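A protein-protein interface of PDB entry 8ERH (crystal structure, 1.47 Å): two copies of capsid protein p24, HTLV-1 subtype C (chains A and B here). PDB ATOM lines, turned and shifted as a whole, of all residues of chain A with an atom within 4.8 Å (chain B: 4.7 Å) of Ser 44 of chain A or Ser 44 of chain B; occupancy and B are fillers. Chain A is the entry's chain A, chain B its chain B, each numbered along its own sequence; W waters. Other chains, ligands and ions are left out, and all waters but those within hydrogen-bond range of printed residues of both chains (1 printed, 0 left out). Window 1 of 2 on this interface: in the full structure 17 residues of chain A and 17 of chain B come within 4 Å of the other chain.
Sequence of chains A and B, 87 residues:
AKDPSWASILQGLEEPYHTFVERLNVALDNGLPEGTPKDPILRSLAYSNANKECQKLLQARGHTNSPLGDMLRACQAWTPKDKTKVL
The side-chain hydroxyl (OG) of Ser 44 of chain A sits at hydrogen-bond distance from the side-chain hydroxyl (OG) of Ser 44 of chain B, 2.7 Å away.
The backbone NH of Leu 45 of chain B is in hydrogen-bond range of the side-chain hydroxyl of Ser 44 of chain A.
OG of Ser 48 of chain B sits at hydrogen-bond distance from OG of Ser 44 of chain A, 2.7 Å away.
The backbone NH (N) of Leu 45 of chain A sits at hydrogen-bond distance from the side-chain hydroxyl (OG) of Ser 44 of chain B (3.4 Å).
The backbone carbonyl oxygen of Ser 44 of chain B sits at hydrogen-bond distance from the side-chain hydroxyl of Ser 48 of chain A.
OG of Ser 48 of chain A lies within hydrogen-bond range of N of Ser 48 of chain B (3.4 Å).
The backbone carbonyl oxygen of Ser 44 of chain A lies within hydrogen-bond range of the side-chain hydroxyl of Ser 48 of chain A (3.3 Å).
OG of Ser 48 of chain B is in hydrogen-bond range of O of Ser 44 of chain B (3.3 Å).
Ile 41 of chain B touches Ile 41 of chain A.
CE1 of Tyr 47 of chain B touches CE2 of Tyr 47 of chain A (3.9 Å).
Tyr 47 of chain A touches Ser 48 of chain B.
Tyr 47 of chain B touches Ser 48 of chain A.
Of the printed residues of chain A, Ser 44 of chain B touches Ser 44, Leu 45 and Ser 48.
Of the printed residues of chain A, Ser 48 of chain B touches Ser 44 (2.7 Å), Tyr 47 (3.9 Å) and Ser 48 (3.4 Å).
Of the printed residues of chain A, Leu 45 of chain B touches Ser 44 (3.4 Å).
Of the printed residues of chain A, Ile 41 of chain B touches Ile 41 (3.8 Å).
Of the printed residues of chain B, Ser 48 of chain A touches Ser 44, Tyr 47 and Ser 48.
The nearest printed residue of chain B that does not touch Ser 44 of chain A is Ile 41 of chain B (5.2 Å).
The nearest printed residue of chain A that does not touch Ser 44 of chain B is Ile 41 of chain A (5.0 Å).
The nearest printed residue of chain B that does not touch Ile 41 of chain A is Ser 44 of chain B (5.0 Å).
Hydrophobic or aromatic side chains of chain A that line the printed part of chain B: Ile 41, Leu 45 and Tyr 47.
Hydrophobic or aromatic side chains of chain B that line the printed part of chain A: Ile 41, Leu 45 and Tyr 47.
Among the printed residues, 10 pairs touch across the chains.
Among the printed residues, no Asp or Glu carboxylate lies within 4 Å of a Lys or Arg side-chain nitrogen of the other chain.
Ile 41 of chain B touches its own counterpart, Ile 41 of chain A.
Ser 44 of chain A touches Leu 45 of chain B, and with the chains exchanged Leu 45 of chain A touches Ser 44 of chain B.
Ser 44 of chain A touches Ser 48 of chain B, and with the chains exchanged Ser 48 of chain A touches Ser 44 of chain B.
Tyr 47 of chain B touches its own counterpart, Tyr 47 of chain A.
Positions printed for both chains: 40, 41, 42, 43, 44, 45, 46, 47 and 48.
Of the 10 pairs that touch across the chains among the printed residues, 10 have their exchanged pair printed and touching as well.
Water W1 bridges OH of Tyr 47 of chain B and OH of Tyr 47 of chain A.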
ATOM      1  N   PRO A  40      15.364 -16.013 -13.157  1.00  0.00           N
ATOM      2  CA  PRO A  40      13.923 -15.865 -13.429  1.00  0.00           C
ATOM      3  C   PRO A  40      13.133 -15.457 -12.201  1.00  0.00           C
ATOM      4  O   PRO A  40      12.138 -14.733 -12.337  1.00  0.00           O
ATOM      5  CB  PRO A  40      13.503 -17.255 -13.945  1.00  0.00           C
ATOM      6  CG  PRO A  40      14.797 -17.900 -14.415  1.00  0.00           C
ATOM      7  CD  PRO A  40      15.854 -17.370 -13.471  1.00  0.00           C
ATOM      8  N   ILE A  41      13.540 -15.911 -11.011  1.00  0.00           N
ATOM      9  CA  ILE A  41      12.828 -15.538  -9.790  1.00  0.00           C
ATOM     10  C   ILE A  41      13.131 -14.090  -9.421  1.00  0.00           C
ATOM     11  O   ILE A  41      12.231 -13.327  -9.033  1.00  0.00           O
ATOM     12  CB  ILE A  41      13.157 -16.535  -8.670  1.00  0.00           C
ATOM     13  CG1 ILE A  41      12.553 -17.903  -9.052  1.00  0.00           C
ATOM     14  CG2 ILE A  41      12.601 -16.064  -7.353  1.00  0.00           C
ATOM     15  CD1 ILE A  41      13.105 -19.033  -8.253  1.00  0.00           C
ATOM     16  N   LEU A  42      14.392 -13.675  -9.556  1.00  0.00           N
ATOM     17  CA  LEU A  42      14.736 -12.267  -9.350  1.00  0.00           C
ATOM     18  C   LEU A  42      13.926 -11.349 -10.270  1.00  0.00           C
ATOM     19  O   LEU A  42      13.360 -10.346  -9.829  1.00  0.00           O
ATOM     20  CB  LEU A  42      16.244 -12.076  -9.549  1.00  0.00           C
ATOM     21  CG  LEU A  42      16.809 -10.664  -9.488  1.00  0.00           C
ATOM     22  CD1 LEU A  42      16.513 -10.014  -8.141  1.00  0.00           C
ATOM     23  CD2 LEU A  42      18.306 -10.687  -9.747  1.00  0.00           C
ATOM     24  N   ARG A  43      13.872 -11.663 -11.558  1.00  0.00           N
ATOM     25  CA  ARG A  43      13.099 -10.843 -12.485  1.00  0.00           C
ATOM     26  C   ARG A  43      11.622 -10.798 -12.107  1.00  0.00           C
ATOM     27  O   ARG A  43      10.975  -9.751 -12.224  1.00  0.00           O
ATOM     28  CB  ARG A  43      13.258 -11.382 -13.912  1.00  0.00           C
ATOM     29  CG  ARG A  43      14.612 -11.147 -14.512  1.00  0.00           C
ATOM     30  CD  ARG A  43      14.598 -11.398 -16.019  1.00  0.00           C
ATOM     31  NE  ARG A  43      13.966 -12.658 -16.406  1.00  0.00           N
ATOM     32  CZ  ARG A  43      14.619 -13.797 -16.585  1.00  0.00           C
ATOM     33  NH1 ARG A  43      15.918 -13.896 -16.339  1.00  0.00           N
ATOM     34  NH2 ARG A  43      13.949 -14.869 -17.000  1.00  0.00           N
ATOM     35  N   SER A  44      11.064 -11.926 -11.672  1.00  0.00           N
ATOM     36  CA  SER A  44       9.657 -11.958 -11.288  1.00  0.00           C
ATOM     37  C   SER A  44       9.394 -11.068 -10.079  1.00  0.00           C
ATOM     38  O   SER A  44       8.496 -10.222 -10.109  1.00  0.00           O
ATOM     39  CB  SER A  44       9.253 -13.379 -10.993  1.00  0.00           C
ATOM     40  OG  SER A  44       7.885 -13.421 -10.643  1.00  0.00           O
ATOM     41  N   LEU A  45      10.169 -11.246  -9.010  1.00  0.00           N
ATOM     42  CA  LEU A  45       9.978 -10.436  -7.803  1.00  0.00           C
ATOM     43  C   LEU A  45      10.255  -8.961  -8.058  1.00  0.00           C
ATOM     44  O   LEU A  45       9.666  -8.092  -7.389  1.00  0.00           O
ATOM     45  CB  LEU A  45      10.881 -10.953  -6.683  1.00  0.00           C
ATOM     46  CG  LEU A  45      10.524 -12.324  -6.144  1.00  0.00           C
ATOM     47  CD1 LEU A  45      11.683 -12.939  -5.402  1.00  0.00           C
ATOM     48  CD2 LEU A  45       9.296 -12.268  -5.251  1.00  0.00           C
ATOM     49  N   ALA A  46      11.170  -8.658  -8.988  1.00  0.00           N
ATOM     50  CA  ALA A  46      11.504  -7.280  -9.328  1.00  0.00           C
ATOM     51  C   ALA A  46      10.334  -6.561  -9.962  1.00  0.00           C
ATOM     52  O   ALA A  46      10.347  -5.325 -10.017  1.00  0.00           O
ATOM     53  CB  ALA A  46      12.766  -7.228 -10.192  1.00  0.00           C
ATOM     54  N   TYR A  47       9.329  -7.301 -10.455  1.00  0.00           N
ATOM     55  CA  TYR A  47       8.057  -6.691 -10.833  1.00  0.00           C
ATOM     56  C   TYR A  47       7.006  -6.817  -9.720  1.00  0.00           C
ATOM     57  O   TYR A  47       6.383  -5.829  -9.310  1.00  0.00           O
ATOM     58  CB  TYR A  47       7.473  -7.339 -12.118  1.00  0.00           C
ATOM     59  CG  TYR A  47       6.183  -6.673 -12.510  1.00  0.00           C
ATOM     60  CD1 TYR A  47       6.198  -5.495 -13.237  1.00  0.00           C
ATOM     61  CD2 TYR A  47       4.969  -7.132 -12.052  1.00  0.00           C
ATOM     62  CE1 TYR A  47       5.053  -4.834 -13.552  1.00  0.00           C
ATOM     63  CE2 TYR A  47       3.795  -6.469 -12.357  1.00  0.00           C
ATOM     64  CZ  TYR A  47       3.860  -5.311 -13.098  1.00  0.00           C
ATOM     65  OH  TYR A  47       2.710  -4.618 -13.400  1.00  0.00           O
ATOM     66  N   SER A  48       6.773  -8.034  -9.224  1.00  0.00           N
ATOM     67  CA  SER A  48       5.643  -8.268  -8.333  1.00  0.00           C
ATOM     68  C   SER A  48       5.778  -7.513  -7.022  1.00  0.00           C
ATOM     69  O   SER A  48       4.766  -7.153  -6.419  1.00  0.00           O
ATOM     70  CB  SER A  48       5.502  -9.762  -8.082  1.00  0.00           C
ATOM     71  OG  SER A  48       5.309 -10.445  -9.303  1.00  0.00           O
ATOM     72  N   PRO B  40       5.451 -19.313  -2.772  1.00  0.00           N
ATOM     73  CA  PRO B  40       5.818 -17.908  -3.024  1.00  0.00           C
ATOM     74  C   PRO B  40       6.296 -17.655  -4.447  1.00  0.00           C
ATOM     75  O   PRO B  40       6.105 -16.549  -4.973  1.00  0.00           O
ATOM     76  CB  PRO B  40       6.908 -17.626  -1.974  1.00  0.00           C
ATOM     77  CG  PRO B  40       7.465 -18.970  -1.633  1.00  0.00           C
ATOM     78  CD  PRO B  40       6.318 -19.952  -1.761  1.00  0.00           C
ATOM     79  N   ILE B  41       6.919 -18.645  -5.085  1.00  0.00           N
ATOM     80  CA  ILE B  41       7.346 -18.471  -6.465  1.00  0.00           C
ATOM     81  C   ILE B  41       6.128 -18.444  -7.380  1.00  0.00           C
ATOM     82  O   ILE B  41       6.032 -17.617  -8.301  1.00  0.00           O
ATOM     83  CB  ILE B  41       8.358 -19.578  -6.826  1.00  0.00           C
ATOM     84  CG1 ILE B  41       9.642 -19.391  -6.004  1.00  0.00           C
ATOM     85  CG2 ILE B  41       8.660 -19.587  -8.320  1.00  0.00           C
ATOM     86  CD1 ILE B  41      10.539 -20.615  -5.979  1.00  0.00           C
ATOM     87  N   LEU B  42       5.172 -19.354  -7.147  1.00  0.00           N
ATOM     88  CA  LEU B  42       3.929 -19.344  -7.910  1.00  0.00           C
ATOM     89  C   LEU B  42       3.234 -17.992  -7.810  1.00  0.00           C
ATOM     90  O   LEU B  42       2.800 -17.420  -8.824  1.00  0.00           O
ATOM     91  CB  LEU B  42       3.000 -20.441  -7.389  1.00  0.00           C
ATOM     92  CG  LEU B  42       1.581 -20.455  -7.946  1.00  0.00           C
ATOM     93  CD1 LEU B  42       1.563 -20.626  -9.454  1.00  0.00           C
ATOM     94  CD2 LEU B  42       0.772 -21.561  -7.262  1.00  0.00           C
ATOM     95  N   ARG B  43       3.122 -17.462  -6.594  1.00  0.00           N
ATOM     96  CA  ARG B  43       2.409 -16.204  -6.436  1.00  0.00           C
ATOM     97  C   ARG B  43       3.123 -15.076  -7.173  1.00  0.00           C
ATOM     98  O   ARG B  43       2.476 -14.222  -7.786  1.00  0.00           O
ATOM     99  CB  ARG B  43       2.218 -15.889  -4.965  1.00  0.00           C
ATOM    100  CG  ARG B  43       1.156 -16.759  -4.308  1.00  0.00           C
ATOM    101  CD  ARG B  43       0.651 -16.137  -3.002  1.00  0.00           C
ATOM    102  NE  ARG B  43       1.733 -15.775  -2.092  1.00  0.00           N
ATOM    103  CZ  ARG B  43       2.346 -16.619  -1.274  1.00  0.00           C
ATOM    104  NH1 ARG B  43       2.000 -17.894  -1.209  1.00  0.00           N
ATOM    105  NH2 ARG B  43       3.329 -16.173  -0.495  1.00  0.00           N
ATOM    106  N   SER B  44       4.457 -15.057  -7.142  1.00  0.00           N
ATOM    107  CA  SER B  44       5.172 -13.986  -7.837  1.00  0.00           C
ATOM    108  C   SER B  44       5.001 -14.111  -9.352  1.00  0.00           C
ATOM    109  O   SER B  44       4.712 -13.127 -10.037  1.00  0.00           O
ATOM    110  CB  SER B  44       6.648 -14.010  -7.481  1.00  0.00           C
ATOM    111  OG  SER B  44       7.309 -12.865  -8.035  1.00  0.00           O
ATOM    112  N   LEU B  45       5.190 -15.315  -9.897  1.00  0.00           N
ATOM    113  CA  LEU B  45       5.108 -15.496 -11.342  1.00  0.00           C
ATOM    114  C   LEU B  45       3.685 -15.332 -11.850  1.00  0.00           C
ATOM    115  O   LEU B  45       3.466 -14.928 -13.011  1.00  0.00           O
ATOM    116  CB  LEU B  45       5.664 -16.875 -11.699  1.00  0.00           C
ATOM    117  CG  LEU B  45       7.173 -17.058 -11.617  1.00  0.00           C
ATOM    118  CD1 LEU B  45       7.528 -18.553 -11.693  1.00  0.00           C
ATOM    119  CD2 LEU B  45       7.906 -16.300 -12.689  1.00  0.00           C
ATOM    120  N   ALA B  46       2.706 -15.692 -11.025  1.00  0.00           N
ATOM    121  CA  ALA B  46       1.318 -15.514 -11.414  1.00  0.00           C
ATOM    122  C   ALA B  46       0.920 -14.051 -11.517  1.00  0.00           C
ATOM    123  O   ALA B  46      -0.157 -13.740 -12.028  1.00  0.00           O
ATOM    124  CB  ALA B  46       0.399 -16.243 -10.450  1.00  0.00           C
ATOM    125  N   TYR B  47       1.759 -13.138 -11.045  1.00  0.00           N
ATOM    126  CA  TYR B  47       1.588 -11.702 -11.212  1.00  0.00           C
ATOM    127  C   TYR B  47       2.507 -11.185 -12.315  1.00  0.00           C
ATOM    128  O   TYR B  47       2.027 -10.593 -13.289  1.00  0.00           O
ATOM    129  CB  TYR B  47       1.874 -11.018  -9.859  1.00  0.00           C
ATOM    130  CG  TYR B  47       1.566  -9.546  -9.708  1.00  0.00           C
ATOM    131  CD1 TYR B  47       0.828  -8.851 -10.649  1.00  0.00           C
ATOM    132  CD2 TYR B  47       1.973  -8.866  -8.586  1.00  0.00           C
ATOM    133  CE1 TYR B  47       0.536  -7.515 -10.486  1.00  0.00           C
ATOM    134  CE2 TYR B  47       1.702  -7.543  -8.418  1.00  0.00           C
ATOM    135  CZ  TYR B  47       0.988  -6.867  -9.361  1.00  0.00           C
ATOM    136  OH  TYR B  47       0.724  -5.530  -9.139  1.00  0.00           O
ATOM    137  N   SER B  48       3.816 -11.468 -12.229  1.00  0.00           N
ATOM    138  CA  SER B  48       4.767 -10.887 -13.175  1.00  0.00           C
ATOM    139  C   SER B  48       4.571 -11.405 -14.593  1.00  0.00           C
ATOM    140  O   SER B  48       4.869 -10.679 -15.541  1.00  0.00           O
ATOM    141  CB  SER B  48       6.204 -11.128 -12.735  1.00  0.00           C
ATOM    142  OG  SER B  48       6.545 -12.491 -12.753  1.00  0.00           O
HETATM  143  O   HOH W   1       0.679  -4.332 -11.540  1.00  0.00           O
